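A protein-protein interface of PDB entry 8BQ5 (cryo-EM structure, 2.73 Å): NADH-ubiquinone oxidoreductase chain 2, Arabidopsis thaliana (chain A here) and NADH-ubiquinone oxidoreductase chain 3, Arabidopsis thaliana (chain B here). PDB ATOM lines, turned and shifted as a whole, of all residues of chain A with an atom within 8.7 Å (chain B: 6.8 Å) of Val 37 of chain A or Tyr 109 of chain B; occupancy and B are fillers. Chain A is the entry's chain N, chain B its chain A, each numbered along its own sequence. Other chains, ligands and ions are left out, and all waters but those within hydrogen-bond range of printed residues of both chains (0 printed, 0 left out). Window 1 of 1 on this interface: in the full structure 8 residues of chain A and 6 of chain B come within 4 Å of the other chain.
The guanidinium group (NH1) of Arg 113 of chain B sits at hydrogen-bond distance from the side-chain hydroxyl (OG) of Ser 40 of chain A, 3.1 Å away.
OE2 of Glu 124 of chain A sits at hydrogen-bond distance from OH of Tyr 109 of chain B, at 2.6 Å.
OE2 of Glu 124 of chain A lies within salt-bridge range of NH2 of Arg 113 of chain B.
O of Val 37 of chain A sits at hydrogen-bond distance from OG1 of Thr 41 of chain A, at 2.8 Å.
OH of Tyr 109 of chain B lies within hydrogen-bond range of NE of Arg 113 of chain B, at 3.5 Å.
OG1 of Thr 41 of chain A lies within hydrogen-bond range of O of Val 38 of chain A.
The backbone carbonyl oxygen (O) of Gly 36 of chain A lies close to the side-chain hydroxyl (OG) of Ser 40 of chain A.
Among the printed residues, pairs that only touch across the chains: Phe 123 of chain A with Arg 113 of chain B (3.1 Å), Thr 41 of chain A with Arg 113 of chain B (3.3 Å), Val 37 of chain A with Tyr 109 of chain B (3.6 Å), Thr 41 of chain A with Lys 112 of chain B (3.6 Å), Val 37 of chain A with Lys 112 of chain B (3.6 Å), Leu 33 of chain A with Ile 105 of chain B (3.8 Å), Leu 33 of chain A with Tyr 109 of chain B (3.8 Å) and Ile 34 of chain A with Ile 105 of chain B (3.9 Å).
Printed residues of chain B within 4 Å of Leu 33 of chain A: Ile 105 (3.8 Å) and Tyr 109 (3.8 Å).
Of the printed residues of chain B, Ile 34 of chain A touches Ile 105 (3.9 Å).
His 35 of chain A touches none of the printed residues of chain B.
Val 37 of chain A touches two residues of chain B.
Printed residues of chain B within 4 Å of Ser 40 of chain A: Arg 113 (3.1 Å).
Printed residues of chain A within 4 Å of Ile 105 of chain B: Leu 33 (3.8 Å) and Ile 34 (3.9 Å).
Of chain A, only Leu 33, Val 37 and Glu 124 come within 4 Å of Tyr 109 of chain B.
Printed residues of chain A within 4 Å of Arg 113 of chain B: Ser 40, Thr 41, Phe 123 and Glu 124.
The nearest residue of chain A that does not touch Tyr 109 of chain B is Phe 123 of chain A (4.3 Å).
The nearest printed residue of chain A that does not touch Arg 113 of chain B is Val 37 of chain A (4.2 Å).
Of the 23 printed residues of chain A, 7 touch a printed residue of chain B.
Hydrophobic or aromatic side chains of chain A that line the printed part of chain B: Leu 33, Ile 34, Val 37 and Phe 123.
Of the 12 printed residues of chain B, 4 touch a printed residue of chain A.
Printed residues of chain B that touch a printed residue of chain A: Ile 105, Tyr 109, Lys 112 and Arg 113.
Hydrophobic or aromatic side chains of chain B within 4 Å of the printed part of chain A: Ile 105 and Tyr 109.
Along chain B the printed residues that touch a printed residue of chain A span positions 105 to 113.
Among the printed residues, 11 pairs touch across the chains.
Among the printed residues, Asp or Glu carboxylates within 4 Å of a Lys or Arg side-chain nitrogen of the other chain: Glu 124 of chain A with Arg 113 of chain B (2.8 Å).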
ATOM      1  N   PHE A  30     -21.633  -2.712 -39.156  1.00  0.00           N
ATOM      2  CA  PHE A  30     -22.289  -3.039 -37.891  1.00  0.00           C
ATOM      3  C   PHE A  30     -21.687  -4.294 -37.264  1.00  0.00           C
ATOM      4  O   PHE A  30     -21.428  -4.337 -36.050  1.00  0.00           O
ATOM      5  CB  PHE A  30     -23.789  -3.218 -38.116  1.00  0.00           C
ATOM      6  CG  PHE A  30     -24.506  -1.943 -38.443  1.00  0.00           C
ATOM      7  CD1 PHE A  30     -23.888  -0.719 -38.255  1.00  0.00           C
ATOM      8  CD2 PHE A  30     -25.795  -1.967 -38.942  1.00  0.00           C
ATOM      9  CE1 PHE A  30     -24.544   0.455 -38.555  1.00  0.00           C
ATOM     10  CE2 PHE A  30     -26.455  -0.796 -39.244  1.00  0.00           C
ATOM     11  CZ  PHE A  30     -25.826   0.416 -39.049  1.00  0.00           C
ATOM     12  N   ILE A  31     -21.450  -5.320 -38.084  1.00  0.00           N
ATOM     13  CA  ILE A  31     -20.834  -6.551 -37.593  1.00  0.00           C
ATOM     14  C   ILE A  31     -19.465  -6.259 -36.991  1.00  0.00           C
ATOM     15  O   ILE A  31     -19.122  -6.764 -35.916  1.00  0.00           O
ATOM     16  CB  ILE A  31     -20.742  -7.591 -38.727  1.00  0.00           C
ATOM     17  CG1 ILE A  31     -22.125  -8.153 -39.059  1.00  0.00           C
ATOM     18  CG2 ILE A  31     -19.781  -8.711 -38.359  1.00  0.00           C
ATOM     19  CD1 ILE A  31     -22.179  -8.895 -40.372  1.00  0.00           C
ATOM     20  N   LEU A  32     -18.662  -5.444 -37.679  1.00  0.00           N
ATOM     21  CA  LEU A  32     -17.319  -5.141 -37.195  1.00  0.00           C
ATOM     22  C   LEU A  32     -17.362  -4.323 -35.909  1.00  0.00           C
ATOM     23  O   LEU A  32     -16.541  -4.534 -35.010  1.00  0.00           O
ATOM     24  CB  LEU A  32     -16.521  -4.412 -38.274  1.00  0.00           C
ATOM     25  CG  LEU A  32     -16.212  -5.261 -39.507  1.00  0.00           C
ATOM     26  CD1 LEU A  32     -15.577  -4.431 -40.612  1.00  0.00           C
ATOM     27  CD2 LEU A  32     -15.333  -6.429 -39.128  1.00  0.00           C
ATOM     28  N   LEU A  33     -18.305  -3.385 -35.809  1.00  0.00           N
ATOM     29  CA  LEU A  33     -18.494  -2.643 -34.565  1.00  0.00           C
ATOM     30  C   LEU A  33     -18.771  -3.587 -33.404  1.00  0.00           C
ATOM     31  O   LEU A  33     -18.137  -3.493 -32.344  1.00  0.00           O
ATOM     32  CB  LEU A  33     -19.645  -1.649 -34.725  1.00  0.00           C
ATOM     33  CG  LEU A  33     -19.898  -0.642 -33.600  1.00  0.00           C
ATOM     34  CD1 LEU A  33     -18.622   0.071 -33.186  1.00  0.00           C
ATOM     35  CD2 LEU A  33     -20.976   0.353 -34.003  1.00  0.00           C
ATOM     36  N   ILE A  34     -19.714  -4.511 -33.590  1.00  0.00           N
ATOM     37  CA  ILE A  34     -20.075  -5.421 -32.505  1.00  0.00           C
ATOM     38  C   ILE A  34     -18.896  -6.321 -32.144  1.00  0.00           C
ATOM     39  O   ILE A  34     -18.581  -6.508 -30.965  1.00  0.00           O
ATOM     40  CB  ILE A  34     -21.326  -6.235 -32.876  1.00  0.00           C
ATOM     41  CG1 ILE A  34     -22.519  -5.301 -33.076  1.00  0.00           C
ATOM     42  CG2 ILE A  34     -21.632  -7.252 -31.797  1.00  0.00           C
ATOM     43  CD1 ILE A  34     -23.576  -5.840 -34.006  1.00  0.00           C
ATOM     44  N   HIS A  35     -18.225  -6.883 -33.151  1.00  0.00           N
ATOM     45  CA  HIS A  35     -17.065  -7.742 -32.913  1.00  0.00           C
ATOM     46  C   HIS A  35     -15.988  -7.007 -32.119  1.00  0.00           C
ATOM     47  O   HIS A  35     -15.480  -7.513 -31.105  1.00  0.00           O
ATOM     48  CB  HIS A  35     -16.530  -8.231 -34.266  1.00  0.00           C
ATOM     49  CG  HIS A  35     -15.194  -8.908 -34.204  1.00  0.00           C
ATOM     50  ND1 HIS A  35     -15.054 -10.267 -34.030  1.00  0.00           N
ATOM     51  CD2 HIS A  35     -13.940  -8.416 -34.334  1.00  0.00           C
ATOM     52  CE1 HIS A  35     -13.771 -10.582 -34.039  1.00  0.00           C
ATOM     53  NE2 HIS A  35     -13.074  -9.476 -34.220  1.00  0.00           N
ATOM     54  N   GLY A  36     -15.653  -5.790 -32.555  1.00  0.00           N
ATOM     55  CA  GLY A  36     -14.617  -5.029 -31.882  1.00  0.00           C
ATOM     56  C   GLY A  36     -14.976  -4.693 -30.450  1.00  0.00           C
ATOM     57  O   GLY A  36     -14.156  -4.839 -29.543  1.00  0.00           O
ATOM     58  N   VAL A  37     -16.212  -4.241 -30.224  1.00  0.00           N
ATOM     59  CA  VAL A  37     -16.581  -3.864 -28.863  1.00  0.00           C
ATOM     60  C   VAL A  37     -16.672  -5.089 -27.960  1.00  0.00           C
ATOM     61  O   VAL A  37     -16.344  -5.011 -26.771  1.00  0.00           O
ATOM     62  CB  VAL A  37     -17.883  -3.040 -28.848  1.00  0.00           C
ATOM     63  CG1 VAL A  37     -19.112  -3.931 -28.900  1.00  0.00           C
ATOM     64  CG2 VAL A  37     -17.920  -2.168 -27.611  1.00  0.00           C
ATOM     65  N   VAL A  38     -17.112  -6.232 -28.488  1.00  0.00           N
ATOM     66  CA  VAL A  38     -17.277  -7.402 -27.638  1.00  0.00           C
ATOM     67  C   VAL A  38     -15.923  -7.961 -27.229  1.00  0.00           C
ATOM     68  O   VAL A  38     -15.725  -8.356 -26.074  1.00  0.00           O
ATOM     69  CB  VAL A  38     -18.151  -8.457 -28.339  1.00  0.00           C
ATOM     70  CG1 VAL A  38     -18.047  -9.791 -27.623  1.00  0.00           C
ATOM     71  CG2 VAL A  38     -19.594  -7.990 -28.386  1.00  0.00           C
ATOM     72  N   PHE A  39     -14.960  -7.994 -28.151  1.00  0.00           N
ATOM     73  CA  PHE A  39     -13.705  -8.647 -27.803  1.00  0.00           C
ATOM     74  C   PHE A  39     -12.628  -7.695 -27.305  1.00  0.00           C
ATOM     75  O   PHE A  39     -11.665  -8.154 -26.683  1.00  0.00           O
ATOM     76  CB  PHE A  39     -13.212  -9.472 -28.989  1.00  0.00           C
ATOM     77  CG  PHE A  39     -14.088 -10.642 -29.266  1.00  0.00           C
ATOM     78  CD1 PHE A  39     -14.049 -11.753 -28.443  1.00  0.00           C
ATOM     79  CD2 PHE A  39     -15.016 -10.602 -30.287  1.00  0.00           C
ATOM     80  CE1 PHE A  39     -14.884 -12.820 -28.666  1.00  0.00           C
ATOM     81  CE2 PHE A  39     -15.856 -11.665 -30.512  1.00  0.00           C
ATOM     82  CZ  PHE A  39     -15.793 -12.773 -29.698  1.00  0.00           C
ATOM     83  N   SER A  40     -12.769  -6.388 -27.524  1.00  0.00           N
ATOM     84  CA  SER A  40     -11.803  -5.457 -26.956  1.00  0.00           C
ATOM     85  C   SER A  40     -11.999  -5.288 -25.454  1.00  0.00           C
ATOM     86  O   SER A  40     -11.042  -4.977 -24.737  1.00  0.00           O
ATOM     87  CB  SER A  40     -11.897  -4.106 -27.659  1.00  0.00           C
ATOM     88  OG  SER A  40     -12.747  -3.227 -26.950  1.00  0.00           O
ATOM     89  N   THR A  41     -13.219  -5.485 -24.959  1.00  0.00           N
ATOM     90  CA  THR A  41     -13.515  -5.357 -23.539  1.00  0.00           C
ATOM     91  C   THR A  41     -13.357  -6.669 -22.784  1.00  0.00           C
ATOM     92  O   THR A  41     -13.605  -6.708 -21.576  1.00  0.00           O
ATOM     93  CB  THR A  41     -14.935  -4.817 -23.341  1.00  0.00           C
ATOM     94  OG1 THR A  41     -15.862  -5.608 -24.093  1.00  0.00           O
ATOM     95  CG2 THR A  41     -15.025  -3.374 -23.800  1.00  0.00           C
ATOM     96  N   SER A  42     -12.934  -7.733 -23.459  1.00  0.00           N
ATOM     97  CA  SER A  42     -12.930  -9.072 -22.881  1.00  0.00           C
ATOM     98  C   SER A  42     -11.714  -9.247 -21.980  1.00  0.00           C
ATOM     99  O   SER A  42     -10.573  -9.052 -22.414  1.00  0.00           O
ATOM    100  CB  SER A  42     -12.944 -10.122 -23.987  1.00  0.00           C
ATOM    101  OG  SER A  42     -13.052 -11.425 -23.448  1.00  0.00           O
ATOM    102  N   TYR A  47      -7.974  -8.058 -23.179  1.00  0.00           N
ATOM    103  CA  TYR A  47      -8.275  -6.807 -23.866  1.00  0.00           C
ATOM    104  C   TYR A  47      -7.356  -6.597 -25.072  1.00  0.00           C
ATOM    105  O   TYR A  47      -6.539  -5.670 -25.083  1.00  0.00           O
ATOM    106  CB  TYR A  47      -8.190  -5.626 -22.911  1.00  0.00           C
ATOM    107  CG  TYR A  47      -8.847  -5.862 -21.572  1.00  0.00           C
ATOM    108  CD1 TYR A  47     -10.197  -5.594 -21.386  1.00  0.00           C
ATOM    109  CD2 TYR A  47      -8.120  -6.340 -20.492  1.00  0.00           C
ATOM    110  CE1 TYR A  47     -10.804  -5.804 -20.167  1.00  0.00           C
ATOM    111  CE2 TYR A  47      -8.719  -6.554 -19.269  1.00  0.00           C
ATOM    112  CZ  TYR A  47     -10.061  -6.284 -19.112  1.00  0.00           C
ATOM    113  OH  TYR A  47     -10.663  -6.493 -17.895  1.00  0.00           O
ATOM    114  N   PRO A  48      -7.463  -7.438 -26.094  1.00  0.00           N
ATOM    115  CA  PRO A  48      -6.527  -7.372 -27.205  1.00  0.00           C
ATOM    116  C   PRO A  48      -6.786  -6.158 -28.077  1.00  0.00           C
ATOM    117  O   PRO A  48      -7.942  -5.765 -28.290  1.00  0.00           O
ATOM    118  CB  PRO A  48      -6.805  -8.674 -27.965  1.00  0.00           C
ATOM    119  CG  PRO A  48      -8.253  -8.923 -27.729  1.00  0.00           C
ATOM    120  CD  PRO A  48      -8.587  -8.347 -26.373  1.00  0.00           C
ATOM    121  N   LEU A  50      -7.506  -4.518 -31.464  1.00  0.00           N
ATOM    122  CA  LEU A  50      -8.214  -5.081 -32.606  1.00  0.00           C
ATOM    123  C   LEU A  50      -8.206  -4.165 -33.818  1.00  0.00           C
ATOM    124  O   LEU A  50      -8.985  -4.389 -34.749  1.00  0.00           O
ATOM    125  CB  LEU A  50      -9.659  -5.419 -32.231  1.00  0.00           C
ATOM    126  CG  LEU A  50      -9.882  -6.460 -31.138  1.00  0.00           C
ATOM    127  CD1 LEU A  50     -11.368  -6.694 -30.954  1.00  0.00           C
ATOM    128  CD2 LEU A  50      -9.164  -7.752 -31.470  1.00  0.00           C
ATOM    129  N   VAL A  54      -9.785  -5.827 -37.135  1.00  0.00           N
ATOM    130  CA  VAL A  54     -10.933  -5.151 -37.726  1.00  0.00           C
ATOM    131  C   VAL A  54     -10.541  -4.487 -39.037  1.00  0.00           C
ATOM    132  O   VAL A  54     -11.345  -4.424 -39.968  1.00  0.00           O
ATOM    133  CB  VAL A  54     -11.528  -4.141 -36.723  1.00  0.00           C
ATOM    134  CG1 VAL A  54     -12.526  -3.219 -37.403  1.00  0.00           C
ATOM    135  CG2 VAL A  54     -12.189  -4.874 -35.569  1.00  0.00           C
ATOM    136  N   ALA A 122      -7.262   1.588 -31.453  1.00  0.00           N
ATOM    137  CA  ALA A 122      -8.688   1.882 -31.590  1.00  0.00           C
ATOM    138  C   ALA A 122      -9.231   1.276 -32.879  1.00  0.00           C
ATOM    139  O   ALA A 122      -8.888   1.725 -33.976  1.00  0.00           O
ATOM    140  CB  ALA A 122      -8.922   3.389 -31.564  1.00  0.00           C
ATOM    141  N   PHE A 123     -10.092   0.262 -32.753  1.00  0.00           N
ATOM    142  CA  PHE A 123     -10.757  -0.280 -33.933  1.00  0.00           C
ATOM    143  C   PHE A 123     -11.840   0.652 -34.459  1.00  0.00           C
ATOM    144  O   PHE A 123     -12.227   0.531 -35.626  1.00  0.00           O
ATOM    145  CB  PHE A 123     -11.368  -1.650 -33.631  1.00  0.00           C
ATOM    146  CG  PHE A 123     -12.589  -1.587 -32.765  1.00  0.00           C
ATOM    147  CD1 PHE A 123     -12.474  -1.576 -31.390  1.00  0.00           C
ATOM    148  CD2 PHE A 123     -13.855  -1.524 -33.328  1.00  0.00           C
ATOM    149  CE1 PHE A 123     -13.594  -1.513 -30.592  1.00  0.00           C
ATOM    150  CE2 PHE A 123     -14.976  -1.456 -32.534  1.00  0.00           C
ATOM    151  CZ  PHE A 123     -14.846  -1.450 -31.164  1.00  0.00           C
ATOM    152  N   GLU A 124     -12.348   1.564 -33.626  1.00  0.00           N
ATOM    153  CA  GLU A 124     -13.398   2.477 -34.065  1.00  0.00           C
ATOM    154  C   GLU A 124     -12.925   3.405 -35.174  1.00  0.00           C
ATOM    155  O   GLU A 124     -13.754   3.973 -35.890  1.00  0.00           O
ATOM    156  CB  GLU A 124     -13.915   3.292 -32.879  1.00  0.00           C
ATOM    157  CG  GLU A 124     -14.599   2.455 -31.811  1.00  0.00           C
ATOM    158  CD  GLU A 124     -13.660   2.033 -30.700  1.00  0.00           C
ATOM    159  OE1 GLU A 124     -12.445   1.916 -30.955  1.00  0.00           O
ATOM    160  OE2 GLU A 124     -14.143   1.813 -29.571  1.00  0.00           O
ATOM    161  N   PHE A 125     -11.612   3.562 -35.329  1.00  0.00           N
ATOM    162  CA  PHE A 125     -11.057   4.306 -36.454  1.00  0.00           C
ATOM    163  C   PHE A 125     -11.477   3.681 -37.784  1.00  0.00           C
ATOM    164  O   PHE A 125     -11.932   4.375 -38.705  1.00  0.00           O
ATOM    165  CB  PHE A 125      -9.536   4.335 -36.294  1.00  0.00           C
ATOM    166  CG  PHE A 125      -8.803   4.955 -37.434  1.00  0.00           C
ATOM    167  CD1 PHE A 125      -8.739   6.328 -37.566  1.00  0.00           C
ATOM    168  CD2 PHE A 125      -8.138   4.164 -38.353  1.00  0.00           C
ATOM    169  CE1 PHE A 125      -8.049   6.898 -38.608  1.00  0.00           C
ATOM    170  CE2 PHE A 125      -7.443   4.731 -39.397  1.00  0.00           C
ATOM    171  CZ  PHE A 125      -7.399   6.100 -39.526  1.00  0.00           C
ATOM    172  N   VAL A 127     -14.061   1.672 -38.237  1.00  0.00           N
ATOM    173  CA  VAL A 127     -15.513   1.771 -38.355  1.00  0.00           C
ATOM    174  C   VAL A 127     -15.922   3.152 -38.853  1.00  0.00           C
ATOM    175  O   VAL A 127     -16.832   3.286 -39.679  1.00  0.00           O
ATOM    176  CB  VAL A 127     -16.181   1.432 -37.009  1.00  0.00           C
ATOM    177  CG1 VAL A 127     -17.692   1.478 -37.137  1.00  0.00           C
ATOM    178  CG2 VAL A 127     -15.730   0.063 -36.527  1.00  0.00           C
ATOM    179  N   LEU A 128     -15.265   4.201 -38.356  1.00  0.00           N
ATOM    180  CA  LEU A 128     -15.589   5.544 -38.823  1.00  0.00           C
ATOM    181  C   LEU A 128     -15.162   5.745 -40.270  1.00  0.00           C
ATOM    182  O   LEU A 128     -15.854   6.427 -41.032  1.00  0.00           O
ATOM    183  CB  LEU A 128     -14.955   6.590 -37.913  1.00  0.00           C
ATOM    184  CG  LEU A 128     -15.516   6.591 -36.490  1.00  0.00           C
ATOM    185  CD1 LEU A 128     -14.496   7.118 -35.502  1.00  0.00           C
ATOM    186  CD2 LEU A 128     -16.799   7.400 -36.426  1.00  0.00           C
ATOM    187  N   THR B 104     -29.924   1.243 -31.700  1.00  0.00           N
ATOM    188  CA  THR B 104     -29.718   0.253 -30.648  1.00  0.00           C
ATOM    189  C   THR B 104     -28.346  -0.403 -30.750  1.00  0.00           C
ATOM    190  O   THR B 104     -27.771  -0.785 -29.729  1.00  0.00           O
ATOM    191  CB  THR B 104     -30.830  -0.798 -30.701  1.00  0.00           C
ATOM    192  OG1 THR B 104     -32.103  -0.145 -30.622  1.00  0.00           O
ATOM    193  CG2 THR B 104     -30.712  -1.779 -29.548  1.00  0.00           C
ATOM    194  N   ILE B 105     -27.805  -0.547 -31.962  1.00  0.00           N
ATOM    195  CA  ILE B 105     -26.400  -0.925 -32.091  1.00  0.00           C
ATOM    196  C   ILE B 105     -25.522   0.108 -31.401  1.00  0.00           C
ATOM    197  O   ILE B 105     -24.596  -0.232 -30.648  1.00  0.00           O
ATOM    198  CB  ILE B 105     -26.019  -1.092 -33.575  1.00  0.00           C
ATOM    199  CG1 ILE B 105     -26.631  -2.369 -34.153  1.00  0.00           C
ATOM    200  CG2 ILE B 105     -24.505  -1.089 -33.748  1.00  0.00           C
ATOM    201  CD1 ILE B 105     -26.592  -3.549 -33.212  1.00  0.00           C
ATOM    202  N   GLY B 106     -25.816   1.390 -31.630  1.00  0.00           N
ATOM    203  CA  GLY B 106     -25.101   2.433 -30.909  1.00  0.00           C
ATOM    204  C   GLY B 106     -25.251   2.323 -29.400  1.00  0.00           C
ATOM    205  O   GLY B 106     -24.280   2.478 -28.654  1.00  0.00           O
ATOM    206  N   PHE B 107     -26.471   2.054 -28.932  1.00  0.00           N
ATOM    207  CA  PHE B 107     -26.711   1.923 -27.497  1.00  0.00           C
ATOM    208  C   PHE B 107     -25.947   0.746 -26.900  1.00  0.00           C
ATOM    209  O   PHE B 107     -25.433   0.835 -25.782  1.00  0.00           O
ATOM    210  CB  PHE B 107     -28.205   1.766 -27.228  1.00  0.00           C
ATOM    211  CG  PHE B 107     -28.567   1.831 -25.776  1.00  0.00           C
ATOM    212  CD1 PHE B 107     -28.294   2.964 -25.030  1.00  0.00           C
ATOM    213  CD2 PHE B 107     -29.175   0.756 -25.153  1.00  0.00           C
ATOM    214  CE1 PHE B 107     -28.629   3.023 -23.693  1.00  0.00           C
ATOM    215  CE2 PHE B 107     -29.511   0.811 -23.816  1.00  0.00           C
ATOM    216  CZ  PHE B 107     -29.238   1.945 -23.087  1.00  0.00           C
ATOM    217  N   LEU B 108     -25.905  -0.379 -27.614  1.00  0.00           N
ATOM    218  CA  LEU B 108     -25.124  -1.523 -27.158  1.00  0.00           C
ATOM    219  C   LEU B 108     -23.650  -1.167 -27.064  1.00  0.00           C
ATOM    220  O   LEU B 108     -22.960  -1.578 -26.123  1.00  0.00           O
ATOM    221  CB  LEU B 108     -25.333  -2.706 -28.101  1.00  0.00           C
ATOM    222  CG  LEU B 108     -24.479  -3.949 -27.859  1.00  0.00           C
ATOM    223  CD1 LEU B 108     -24.649  -4.454 -26.436  1.00  0.00           C
ATOM    224  CD2 LEU B 108     -24.827  -5.033 -28.864  1.00  0.00           C
ATOM    225  N   TYR B 109     -23.151  -0.403 -28.037  1.00  0.00           N
ATOM    226  CA  TYR B 109     -21.779   0.087 -27.955  1.00  0.00           C
ATOM    227  C   TYR B 109     -21.582   0.941 -26.705  1.00  0.00           C
ATOM    228  O   TYR B 109     -20.545   0.855 -26.037  1.00  0.00           O
ATOM    229  CB  TYR B 109     -21.428   0.874 -29.217  1.00  0.00           C
ATOM    230  CG  TYR B 109     -20.054   1.493 -29.177  1.00  0.00           C
ATOM    231  CD1 TYR B 109     -18.922   0.730 -29.415  1.00  0.00           C
ATOM    232  CD2 TYR B 109     -19.888   2.837 -28.882  1.00  0.00           C
ATOM    233  CE1 TYR B 109     -17.666   1.289 -29.372  1.00  0.00           C
ATOM    234  CE2 TYR B 109     -18.637   3.405 -28.836  1.00  0.00           C
ATOM    235  CZ  TYR B 109     -17.528   2.628 -29.081  1.00  0.00           C
ATOM    236  OH  TYR B 109     -16.278   3.194 -29.036  1.00  0.00           O
ATOM    237  N   GLU B 110     -22.571   1.780 -26.380  1.00  0.00           N
ATOM    238  CA  GLU B 110     -22.509   2.579 -25.154  1.00  0.00           C
ATOM    239  C   GLU B 110     -22.419   1.691 -23.924  1.00  0.00           C
ATOM    240  O   GLU B 110     -21.574   1.903 -23.047  1.00  0.00           O
ATOM    241  CB  GLU B 110     -23.749   3.468 -25.027  1.00  0.00           C
ATOM    242  CG  GLU B 110     -24.055   4.400 -26.181  1.00  0.00           C
ATOM    243  CD  GLU B 110     -23.051   5.507 -26.353  1.00  0.00           C
ATOM    244  OE1 GLU B 110     -23.447   6.603 -26.797  1.00  0.00           O
ATOM    245  OE2 GLU B 110     -21.873   5.296 -26.050  1.00  0.00           O
ATOM    246  N   TRP B 111     -23.319   0.714 -23.835  1.00  0.00           N
ATOM    247  CA  TRP B 111     -23.353  -0.218 -22.716  1.00  0.00           C
ATOM    248  C   TRP B 111     -22.006  -0.900 -22.522  1.00  0.00           C
ATOM    249  O   TRP B 111     -21.463  -0.923 -21.412  1.00  0.00           O
ATOM    250  CB  TRP B 111     -24.442  -1.258 -22.964  1.00  0.00           C
ATOM    251  CG  TRP B 111     -24.890  -2.022 -21.767  1.00  0.00           C
ATOM    252  CD1 TRP B 111     -24.103  -2.711 -20.893  1.00  0.00           C
ATOM    253  CD2 TRP B 111     -26.240  -2.244 -21.350  1.00  0.00           C
ATOM    254  NE1 TRP B 111     -24.877  -3.320 -19.939  1.00  0.00           N
ATOM    255  CE2 TRP B 111     -26.194  -3.050 -20.199  1.00  0.00           C
ATOM    256  CE3 TRP B 111     -27.483  -1.824 -21.831  1.00  0.00           C
ATOM    257  CZ2 TRP B 111     -27.341  -3.445 -19.520  1.00  0.00           C
ATOM    258  CZ3 TRP B 111     -28.619  -2.219 -21.157  1.00  0.00           C
ATOM    259  CH2 TRP B 111     -28.541  -3.020 -20.014  1.00  0.00           C
ATOM    260  N   LYS B 112     -21.452  -1.462 -23.598  1.00  0.00           N
ATOM    261  CA  LYS B 112     -20.244  -2.273 -23.468  1.00  0.00           C
ATOM    262  C   LYS B 112     -19.033  -1.424 -23.104  1.00  0.00           C
ATOM    263  O   LYS B 112     -18.064  -1.934 -22.534  1.00  0.00           O
ATOM    264  CB  LYS B 112     -19.989  -3.042 -24.761  1.00  0.00           C
ATOM    265  CG  LYS B 112     -21.084  -4.020 -25.128  1.00  0.00           C
ATOM    266  CD  LYS B 112     -21.176  -5.169 -24.147  1.00  0.00           C
ATOM    267  CE  LYS B 112     -20.139  -6.234 -24.451  1.00  0.00           C
ATOM    268  NZ  LYS B 112     -19.510  -6.785 -23.222  1.00  0.00           N
ATOM    269  N   ARG B 113     -19.066  -0.130 -23.421  1.00  0.00           N
ATOM    270  CA  ARG B 113     -17.939   0.744 -23.132  1.00  0.00           C
ATOM    271  C   ARG B 113     -18.011   1.384 -21.752  1.00  0.00           C
ATOM    272  O   ARG B 113     -17.136   2.186 -21.414  1.00  0.00           O
ATOM    273  CB  ARG B 113     -17.833   1.843 -24.191  1.00  0.00           C
ATOM    274  CG  ARG B 113     -17.132   1.403 -25.461  1.00  0.00           C
ATOM    275  CD  ARG B 113     -15.639   1.632 -25.366  1.00  0.00           C
ATOM    276  NE  ARG B 113     -14.936   1.168 -26.554  1.00  0.00           N
ATOM    277  CZ  ARG B 113     -14.198   0.068 -26.609  1.00  0.00           C
ATOM    278  NH1 ARG B 113     -14.064  -0.727 -25.562  1.00  0.00           N
ATOM    279  NH2 ARG B 113     -13.569  -0.235 -27.739  1.00  0.00           N
ATOM    280  N   GLY B 114     -19.021   1.060 -20.953  1.00  0.00           N
ATOM    281  CA  GLY B 114     -19.127   1.599 -19.615  1.00  0.00           C
ATOM    282  C   GLY B 114     -19.686   2.999 -19.512  1.00  0.00           C
ATOM    283  O   GLY B 114     -19.461   3.662 -18.494  1.00  0.00           O
ATOM    284  N   ALA B 115     -20.396   3.483 -20.533  1.00  0.00           N
ATOM    285  CA  ALA B 115     -20.987   4.812 -20.451  1.00  0.00           C
ATOM    286  C   ALA B 115     -22.222   4.846 -19.562  1.00  0.00           C
ATOM    287  O   ALA B 115     -22.606   5.924 -19.098  1.00  0.00           O
ATOM    288  CB  ALA B 115     -21.346   5.322 -21.847  1.00  0.00           C
